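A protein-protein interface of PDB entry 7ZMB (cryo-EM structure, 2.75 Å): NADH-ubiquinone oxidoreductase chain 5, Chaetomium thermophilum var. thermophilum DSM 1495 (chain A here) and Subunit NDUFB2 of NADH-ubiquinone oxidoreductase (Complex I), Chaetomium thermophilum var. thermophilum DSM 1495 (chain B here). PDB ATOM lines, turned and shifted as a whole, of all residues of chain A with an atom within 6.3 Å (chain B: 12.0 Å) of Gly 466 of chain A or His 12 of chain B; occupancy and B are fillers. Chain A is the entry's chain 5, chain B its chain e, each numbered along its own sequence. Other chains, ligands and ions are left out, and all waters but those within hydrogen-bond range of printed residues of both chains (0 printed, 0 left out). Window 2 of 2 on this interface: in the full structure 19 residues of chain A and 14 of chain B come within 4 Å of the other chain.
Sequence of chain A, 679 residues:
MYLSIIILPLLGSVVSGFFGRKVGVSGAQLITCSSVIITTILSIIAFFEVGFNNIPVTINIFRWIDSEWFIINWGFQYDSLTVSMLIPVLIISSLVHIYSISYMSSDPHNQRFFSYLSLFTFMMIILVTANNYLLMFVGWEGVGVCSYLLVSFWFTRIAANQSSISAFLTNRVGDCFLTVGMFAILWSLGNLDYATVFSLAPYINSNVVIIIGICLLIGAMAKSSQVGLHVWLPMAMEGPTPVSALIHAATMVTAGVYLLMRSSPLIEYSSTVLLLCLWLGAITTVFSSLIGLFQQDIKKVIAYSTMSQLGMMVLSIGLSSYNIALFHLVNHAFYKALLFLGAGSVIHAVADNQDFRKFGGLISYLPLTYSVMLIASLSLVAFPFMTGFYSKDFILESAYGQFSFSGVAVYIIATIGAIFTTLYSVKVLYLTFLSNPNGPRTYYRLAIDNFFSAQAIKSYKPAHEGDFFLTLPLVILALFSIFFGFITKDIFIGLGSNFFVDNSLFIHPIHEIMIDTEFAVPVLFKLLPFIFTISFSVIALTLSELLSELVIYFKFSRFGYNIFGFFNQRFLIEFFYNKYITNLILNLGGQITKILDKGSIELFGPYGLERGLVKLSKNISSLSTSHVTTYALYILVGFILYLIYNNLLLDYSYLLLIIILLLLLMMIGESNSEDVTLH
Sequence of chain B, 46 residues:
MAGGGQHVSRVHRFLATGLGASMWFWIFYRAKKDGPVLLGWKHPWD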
ATOM      1  N   SER A 102     -21.527 -21.154  23.708  1.00  0.00           N
ATOM      2  CA  SER A 102     -20.932 -19.847  23.933  1.00  0.00           C
ATOM      3  C   SER A 102     -21.980 -18.828  24.348  1.00  0.00           C
ATOM      4  O   SER A 102     -21.714 -17.960  25.184  1.00  0.00           O
ATOM      5  CB  SER A 102     -20.212 -19.384  22.669  1.00  0.00           C
ATOM      6  OG  SER A 102     -19.763 -18.045  22.792  1.00  0.00           O
ATOM      7  N   SER A 345     -23.711 -12.706  17.479  1.00  0.00           N
ATOM      8  CA  SER A 345     -22.365 -12.332  17.981  1.00  0.00           C
ATOM      9  C   SER A 345     -22.293 -10.808  18.078  1.00  0.00           C
ATOM     10  O   SER A 345     -21.570 -10.315  18.961  1.00  0.00           O
ATOM     11  CB  SER A 345     -21.287 -12.886  17.094  1.00  0.00           C
ATOM     12  OG  SER A 345     -21.605 -12.690  15.728  1.00  0.00           O
ATOM     13  N   HIS A 348     -23.761  -9.839  21.363  1.00  0.00           N
ATOM     14  CA  HIS A 348     -22.847 -10.215  22.473  1.00  0.00           C
ATOM     15  C   HIS A 348     -21.709  -9.194  22.565  1.00  0.00           C
ATOM     16  O   HIS A 348     -21.240  -8.939  23.691  1.00  0.00           O
ATOM     17  CB  HIS A 348     -22.334 -11.647  22.275  1.00  0.00           C
ATOM     18  CG  HIS A 348     -21.498 -12.150  23.404  1.00  0.00           C
ATOM     19  ND1 HIS A 348     -22.049 -12.595  24.589  1.00  0.00           N
ATOM     20  CD2 HIS A 348     -20.160 -12.282  23.532  1.00  0.00           C
ATOM     21  CE1 HIS A 348     -21.086 -12.978  25.402  1.00  0.00           C
ATOM     22  NE2 HIS A 348     -19.917 -12.796  24.777  1.00  0.00           N
ATOM     23  N   PRO A 367     -14.212  -8.264  12.444  1.00  0.00           N
ATOM     24  CA  PRO A 367     -13.904  -8.558  11.039  1.00  0.00           C
ATOM     25  C   PRO A 367     -14.594  -9.818  10.541  1.00  0.00           C
ATOM     26  O   PRO A 367     -15.226  -9.808   9.480  1.00  0.00           O
ATOM     27  CB  PRO A 367     -12.379  -8.709  11.041  1.00  0.00           C
ATOM     28  CG  PRO A 367     -12.053  -9.145  12.424  1.00  0.00           C
ATOM     29  CD  PRO A 367     -13.042  -8.455  13.319  1.00  0.00           C
ATOM     30  N   LEU A 368     -14.480 -10.910  11.299  1.00  0.00           N
ATOM     31  CA  LEU A 368     -15.102 -12.165  10.888  1.00  0.00           C
ATOM     32  C   LEU A 368     -16.618 -12.040  10.846  1.00  0.00           C
ATOM     33  O   LEU A 368     -17.265 -12.534   9.915  1.00  0.00           O
ATOM     34  CB  LEU A 368     -14.684 -13.291  11.831  1.00  0.00           C
ATOM     35  CG  LEU A 368     -15.289 -14.662  11.537  1.00  0.00           C
ATOM     36  CD1 LEU A 368     -14.950 -15.102  10.124  1.00  0.00           C
ATOM     37  CD2 LEU A 368     -14.801 -15.683  12.549  1.00  0.00           C
ATOM     38  N   THR A 369     -17.200 -11.375  11.845  1.00  0.00           N
ATOM     39  CA  THR A 369     -18.651 -11.243  11.900  1.00  0.00           C
ATOM     40  C   THR A 369     -19.180 -10.469  10.700  1.00  0.00           C
ATOM     41  O   THR A 369     -20.230 -10.811  10.143  1.00  0.00           O
ATOM     42  CB  THR A 369     -19.062 -10.561  13.202  1.00  0.00           C
ATOM     43  OG1 THR A 369     -18.471 -11.253  14.310  1.00  0.00           O
ATOM     44  CG2 THR A 369     -20.569 -10.578  13.354  1.00  0.00           C
ATOM     45  N   HIS A 464     -15.128  -7.187  21.553  1.00  0.00           N
ATOM     46  CA  HIS A 464     -14.394  -8.233  20.861  1.00  0.00           C
ATOM     47  C   HIS A 464     -15.353  -9.308  20.359  1.00  0.00           C
ATOM     48  O   HIS A 464     -16.500  -9.408  20.801  1.00  0.00           O
ATOM     49  CB  HIS A 464     -13.343  -8.853  21.781  1.00  0.00           C
ATOM     50  CG  HIS A 464     -13.919  -9.662  22.900  1.00  0.00           C
ATOM     51  ND1 HIS A 464     -14.966  -9.217  23.679  1.00  0.00           N
ATOM     52  CD2 HIS A 464     -13.592 -10.887  23.376  1.00  0.00           C
ATOM     53  CE1 HIS A 464     -15.261 -10.134  24.584  1.00  0.00           C
ATOM     54  NE2 HIS A 464     -14.441 -11.157  24.421  1.00  0.00           N
ATOM     55  N   GLU A 465     -14.869 -10.118  19.422  1.00  0.00           N
ATOM     56  CA  GLU A 465     -15.673 -11.215  18.908  1.00  0.00           C
ATOM     57  C   GLU A 465     -15.726 -12.351  19.928  1.00  0.00           C
ATOM     58  O   GLU A 465     -15.087 -12.312  20.984  1.00  0.00           O
ATOM     59  CB  GLU A 465     -15.123 -11.707  17.572  1.00  0.00           C
ATOM     60  CG  GLU A 465     -15.478 -10.825  16.388  1.00  0.00           C
ATOM     61  CD  GLU A 465     -15.066 -11.438  15.064  1.00  0.00           C
ATOM     62  OE1 GLU A 465     -14.368 -12.474  15.082  1.00  0.00           O
ATOM     63  OE2 GLU A 465     -15.446 -10.891  14.008  1.00  0.00           O
ATOM     64  N   GLY A 466     -16.502 -13.380  19.603  1.00  0.00           N
ATOM     65  CA  GLY A 466     -16.699 -14.501  20.493  1.00  0.00           C
ATOM     66  C   GLY A 466     -15.582 -15.522  20.402  1.00  0.00           C
ATOM     67  O   GLY A 466     -14.562 -15.331  19.736  1.00  0.00           O
ATOM     68  N   ASP A 467     -15.791 -16.636  21.095  1.00  0.00           N
ATOM     69  CA  ASP A 467     -14.821 -17.712  21.171  1.00  0.00           C
ATOM     70  C   ASP A 467     -15.085 -18.744  20.076  1.00  0.00           C
ATOM     71  O   ASP A 467     -15.869 -18.516  19.152  1.00  0.00           O
ATOM     72  CB  ASP A 467     -14.845 -18.341  22.567  1.00  0.00           C
ATOM     73  CG  ASP A 467     -16.044 -19.239  22.781  1.00  0.00           C
ATOM     74  OD1 ASP A 467     -17.122 -18.939  22.226  1.00  0.00           O
ATOM     75  OD2 ASP A 467     -15.907 -20.251  23.499  1.00  0.00           O
ATOM     76  N   PHE A 468     -14.420 -19.896  20.185  1.00  0.00           N
ATOM     77  CA  PHE A 468     -14.520 -20.931  19.161  1.00  0.00           C
ATOM     78  C   PHE A 468     -15.948 -21.436  19.005  1.00  0.00           C
ATOM     79  O   PHE A 468     -16.426 -21.622  17.881  1.00  0.00           O
ATOM     80  CB  PHE A 468     -13.582 -22.085  19.506  1.00  0.00           C
ATOM     81  CG  PHE A 468     -13.623 -23.219  18.521  1.00  0.00           C
ATOM     82  CD1 PHE A 468     -12.999 -23.109  17.291  1.00  0.00           C
ATOM     83  CD2 PHE A 468     -14.281 -24.397  18.831  1.00  0.00           C
ATOM     84  CE1 PHE A 468     -13.032 -24.154  16.385  1.00  0.00           C
ATOM     85  CE2 PHE A 468     -14.319 -25.445  17.930  1.00  0.00           C
ATOM     86  CZ  PHE A 468     -13.693 -25.322  16.706  1.00  0.00           C
ATOM     87  N   PHE A 469     -16.641 -21.666  20.122  1.00  0.00           N
ATOM     88  CA  PHE A 469     -17.985 -22.226  20.055  1.00  0.00           C
ATOM     89  C   PHE A 469     -18.957 -21.280  19.358  1.00  0.00           C
ATOM     90  O   PHE A 469     -19.946 -21.731  18.770  1.00  0.00           O
ATOM     91  CB  PHE A 469     -18.471 -22.563  21.462  1.00  0.00           C
ATOM     92  CG  PHE A 469     -17.974 -23.885  21.968  1.00  0.00           C
ATOM     93  CD1 PHE A 469     -16.743 -23.980  22.598  1.00  0.00           C
ATOM     94  CD2 PHE A 469     -18.726 -25.032  21.811  1.00  0.00           C
ATOM     95  CE1 PHE A 469     -16.278 -25.193  23.061  1.00  0.00           C
ATOM     96  CE2 PHE A 469     -18.266 -26.249  22.272  1.00  0.00           C
ATOM     97  CZ  PHE A 469     -17.040 -26.330  22.898  1.00  0.00           C
ATOM     98  N   LEU A 470     -18.688 -19.977  19.403  1.00  0.00           N
ATOM     99  CA  LEU A 470     -19.543 -18.982  18.766  1.00  0.00           C
ATOM    100  C   LEU A 470     -19.218 -18.771  17.297  1.00  0.00           C
ATOM    101  O   LEU A 470     -20.121 -18.468  16.508  1.00  0.00           O
ATOM    102  CB  LEU A 470     -19.422 -17.645  19.499  1.00  0.00           C
ATOM    103  CG  LEU A 470     -20.576 -16.653  19.362  1.00  0.00           C
ATOM    104  CD1 LEU A 470     -21.855 -17.279  19.847  1.00  0.00           C
ATOM    105  CD2 LEU A 470     -20.277 -15.383  20.139  1.00  0.00           C
ATOM    106  N   THR A 471     -17.952 -18.916  16.910  1.00  0.00           N
ATOM    107  CA  THR A 471     -17.518 -18.625  15.550  1.00  0.00           C
ATOM    108  C   THR A 471     -17.545 -19.836  14.631  1.00  0.00           C
ATOM    109  O   THR A 471     -17.684 -19.669  13.415  1.00  0.00           O
ATOM    110  CB  THR A 471     -16.101 -18.045  15.558  1.00  0.00           C
ATOM    111  OG1 THR A 471     -15.206 -18.982  16.170  1.00  0.00           O
ATOM    112  CG2 THR A 471     -16.064 -16.739  16.334  1.00  0.00           C
ATOM    113  N   SER B   9      -4.700 -12.575  18.851  1.00  0.00           N
ATOM    114  CA  SER B   9      -5.827 -13.275  18.249  1.00  0.00           C
ATOM    115  C   SER B   9      -5.968 -12.919  16.772  1.00  0.00           C
ATOM    116  O   SER B   9      -7.053 -12.567  16.310  1.00  0.00           O
ATOM    117  CB  SER B   9      -7.121 -12.949  18.997  1.00  0.00           C
ATOM    118  OG  SER B   9      -7.037 -13.340  20.356  1.00  0.00           O
ATOM    119  N   ARG B  10      -4.859 -13.012  16.037  1.00  0.00           N
ATOM    120  CA  ARG B  10      -4.866 -12.704  14.613  1.00  0.00           C
ATOM    121  C   ARG B  10      -5.544 -13.780  13.777  1.00  0.00           C
ATOM    122  O   ARG B  10      -5.779 -13.554  12.586  1.00  0.00           O
ATOM    123  CB  ARG B  10      -3.434 -12.496  14.115  1.00  0.00           C
ATOM    124  N   VAL B  11      -5.857 -14.938  14.364  1.00  0.00           N
ATOM    125  CA  VAL B  11      -6.498 -16.006  13.604  1.00  0.00           C
ATOM    126  C   VAL B  11      -7.891 -15.589  13.150  1.00  0.00           C
ATOM    127  O   VAL B  11      -8.379 -16.055  12.112  1.00  0.00           O
ATOM    128  CB  VAL B  11      -6.532 -17.305  14.434  1.00  0.00           C
ATOM    129  CG1 VAL B  11      -7.407 -17.139  15.666  1.00  0.00           C
ATOM    130  CG2 VAL B  11      -7.001 -18.477  13.584  1.00  0.00           C
ATOM    131  N   HIS B  12      -8.552 -14.707  13.903  1.00  0.00           N
ATOM    132  CA  HIS B  12      -9.875 -14.238  13.504  1.00  0.00           C
ATOM    133  C   HIS B  12      -9.816 -13.491  12.178  1.00  0.00           C
ATOM    134  O   HIS B  12     -10.674 -13.685  11.309  1.00  0.00           O
ATOM    135  CB  HIS B  12     -10.466 -13.345  14.594  1.00  0.00           C
ATOM    136  CG  HIS B  12     -11.223 -14.095  15.644  1.00  0.00           C
ATOM    137  ND1 HIS B  12     -11.736 -13.485  16.768  1.00  0.00           N
ATOM    138  CD2 HIS B  12     -11.554 -15.404  15.742  1.00  0.00           C
ATOM    139  CE1 HIS B  12     -12.351 -14.386  17.514  1.00  0.00           C
ATOM    140  NE2 HIS B  12     -12.255 -15.558  16.913  1.00  0.00           N
ATOM    141  N   ARG B  13      -8.807 -12.636  12.002  1.00  0.00           N
ATOM    142  CA  ARG B  13      -8.681 -11.891  10.755  1.00  0.00           C
ATOM    143  C   ARG B  13      -8.418 -12.823   9.580  1.00  0.00           C
ATOM    144  O   ARG B  13      -8.924 -12.597   8.474  1.00  0.00           O
ATOM    145  CB  ARG B  13      -7.571 -10.848  10.875  1.00  0.00           C
ATOM    146  CG  ARG B  13      -7.744  -9.651   9.956  1.00  0.00           C
ATOM    147  CD  ARG B  13      -7.091  -8.409  10.537  1.00  0.00           C
ATOM    148  NE  ARG B  13      -7.371  -8.261  11.962  1.00  0.00           N
ATOM    149  CZ  ARG B  13      -6.931  -7.252  12.708  1.00  0.00           C
ATOM    150  NH1 ARG B  13      -7.235  -7.199  13.998  1.00  0.00           N
ATOM    151  NH2 ARG B  13      -6.190  -6.296  12.165  1.00  0.00           N
ATOM    152  N   PHE B  14      -7.625 -13.875   9.797  1.00  0.00           N
ATOM    153  CA  PHE B  14      -7.365 -14.834   8.729  1.00  0.00           C
ATOM    154  C   PHE B  14      -8.646 -15.522   8.281  1.00  0.00           C
ATOM    155  O   PHE B  14      -8.876 -15.700   7.080  1.00  0.00           O
ATOM    156  CB  PHE B  14      -6.334 -15.867   9.182  1.00  0.00           C
ATOM    157  CG  PHE B  14      -5.983 -16.870   8.123  1.00  0.00           C
ATOM    158  CD1 PHE B  14      -5.153 -16.525   7.071  1.00  0.00           C
ATOM    159  CD2 PHE B  14      -6.489 -18.159   8.178  1.00  0.00           C
ATOM    160  CE1 PHE B  14      -4.832 -17.449   6.094  1.00  0.00           C
ATOM    161  CE2 PHE B  14      -6.170 -19.085   7.206  1.00  0.00           C
ATOM    162  CZ  PHE B  14      -5.340 -18.730   6.161  1.00  0.00           C
ATOM    163  N   LEU B  15      -9.489 -15.924   9.234  1.00  0.00           N
ATOM    164  CA  LEU B  15     -10.780 -16.500   8.872  1.00  0.00           C
ATOM    165  C   LEU B  15     -11.666 -15.467   8.190  1.00  0.00           C
ATOM    166  O   LEU B  15     -12.416 -15.799   7.264  1.00  0.00           O
ATOM    167  CB  LEU B  15     -11.473 -17.070  10.110  1.00  0.00           C
ATOM    168  CG  LEU B  15     -11.193 -18.532  10.469  1.00  0.00           C
ATOM    169  CD1 LEU B  15     -11.644 -19.453   9.346  1.00  0.00           C
ATOM    170  CD2 LEU B  15      -9.725 -18.760  10.797  1.00  0.00           C
ATOM    171  N   ALA B  16     -11.596 -14.211   8.635  1.00  0.00           N
ATOM    172  CA  ALA B  16     -12.385 -13.155   8.009  1.00  0.00           C
ATOM    173  C   ALA B  16     -12.005 -12.982   6.546  1.00  0.00           C
ATOM    174  O   ALA B  16     -12.867 -13.002   5.660  1.00  0.00           O
ATOM    175  CB  ALA B  16     -12.201 -11.843   8.771  1.00  0.00           C
ATOM    176  N   THR B  17     -10.711 -12.815   6.271  1.00  0.00           N
ATOM    177  CA  THR B  17     -10.268 -12.672   4.890  1.00  0.00           C
ATOM    178  C   THR B  17     -10.294 -14.002   4.153  1.00  0.00           C
ATOM    179  O   THR B  17     -10.576 -14.034   2.951  1.00  0.00           O
ATOM    180  CB  THR B  17      -8.866 -12.069   4.843  1.00  0.00           C
ATOM    181  OG1 THR B  17      -7.947 -12.941   5.513  1.00  0.00           O
ATOM    182  CG2 THR B  17      -8.851 -10.707   5.519  1.00  0.00           C
ATOM    183  N   GLY B  18     -10.003 -15.104   4.848  1.00  0.00           N
ATOM    184  CA  GLY B  18      -9.985 -16.400   4.188  1.00  0.00           C
ATOM    185  C   GLY B  18     -11.334 -16.770   3.604  1.00  0.00           C
ATOM    186  O   GLY B  18     -11.430 -17.207   2.455  1.00  0.00           O
ATOM    187  N   LEU B  19     -12.398 -16.556   4.321  1.00  0.00           N
ATOM    188  CA  LEU B  19     -13.746 -16.798   3.748  1.00  0.00           C
ATOM    189  C   LEU B  19     -13.990 -15.692   2.723  1.00  0.00           C
ATOM    190  O   LEU B  19     -14.594 -15.966   1.678  1.00  0.00           O
ATOM    191  CB  LEU B  19     -14.778 -16.750   4.871  1.00  0.00           C
ATOM    192  CG  LEU B  19     -14.678 -17.877   5.897  1.00  0.00           C
ATOM    193  CD1 LEU B  19     -15.603 -17.619   7.075  1.00  0.00           C
ATOM    194  CD2 LEU B  19     -14.986 -19.221   5.258  1.00  0.00           C
ATOM    195  N   GLY B  20     -13.555 -14.450   3.054  1.00  0.00           N
ATOM    196  CA  GLY B  20     -13.654 -13.403   2.057  1.00  0.00           C
ATOM    197  C   GLY B  20     -12.821 -13.659   0.821  1.00  0.00           C
ATOM    198  O   GLY B  20     -13.129 -13.116  -0.244  1.00  0.00           O
ATOM    199  N   ALA B  21     -11.768 -14.469   0.940  1.00  0.00           N
ATOM    200  CA  ALA B  21     -10.978 -14.869  -0.217  1.00  0.00           C
ATOM    201  C   ALA B  21     -11.613 -16.036  -0.961  1.00  0.00           C
ATOM    202  O   ALA B  21     -11.530 -16.102  -2.191  1.00  0.00           O
ATOM    203  CB  ALA B  21      -9.556 -15.237   0.210  1.00  0.00           C
ATOM    204  N   SER B  22     -12.235 -16.965  -0.233  1.00  0.00           N
ATOM    205  CA  SER B  22     -12.991 -18.026  -0.889  1.00  0.00           C
ATOM    206  C   SER B  22     -14.133 -17.438  -1.704  1.00  0.00           C
ATOM    207  O   SER B  22     -14.349 -17.816  -2.861  1.00  0.00           O
ATOM    208  CB  SER B  22     -13.515 -19.015   0.151  1.00  0.00           C
ATOM    209  OG  SER B  22     -14.408 -18.380   1.048  1.00  0.00           O
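The side-chain carboxylate (OE1) of Glu 465 of chain A is in hydrogen-bond range of a ring nitrogen (ND1) of His 12 of chain B (3.3 Å).
The side-chain carboxylate of Glu 465 of chain A lies within hydrogen-bond range of the backbone NH of Leu 368 of chain A, 2.9 Å away. The backbone NH of Thr 369 of chain A is in hydrogen-bond range of the side-chain carboxylate of Glu 465 of chain A, at 2.8 Å.
CB of Ala 16 of chain B touches C of Pro 367 of chain A, at 3.6 Å. Leu 15 of chain B touches Leu 368 of chain A. N of Leu 368 of chain A touches CB of Ala 16 of chain B, at 3.5 Å. CE1 of His 12 of chain B touches O of Gly 466 of chain A, 3.3 Å away.
Printed residues of chain B within 4 Å of Gly 466 of chain A: His 12. No residue of chain B comes within 4 Å of Ser 345 of chain A. Of chain B, only Ala 16 (3.6 Å) comes within 4 Å of Pro 367 of chain A. No residue of chain B comes within 4 Å of His 464 of chain A. Glu 465 of chain A touches just one residue of chain B: His 12. No residue of chain B comes within 4 Å of Asp 467 of chain A. No residue of chain B comes within 4 Å of Leu 470 of chain A. No residue of chain B comes within 4 Å of Thr 471 of chain A. Of the printed residues of chain A, Ala 16 of chain B touches Pro 367 (3.6 Å) and Leu 368 (3.5 Å). Of the printed residues of chain A, Leu 15 of chain B touches Leu 368. Of the printed residues of chain B, Leu 368 of chain A touches Leu 15 (3.8 Å) and Ala 16 (3.5 Å). His 348 of chain A touches none of the printed residues of chain B. Leu 19 of chain B touches none of the printed residues of chain A. The nearest residue of chain B that does not touch Gly 466 of chain A is Ser 9 of chain B (7.8 Å). The nearest printed residue of chain A that does not touch Ala 16 of chain B is Thr 369 of chain A (5.9 Å).
Printed residues of chain A that touch a printed residue of chain B: Pro 367, Leu 368, Glu 465 and Gly 466. Along chain A the printed residues that touch a printed residue of chain B span positions 367 to 466.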
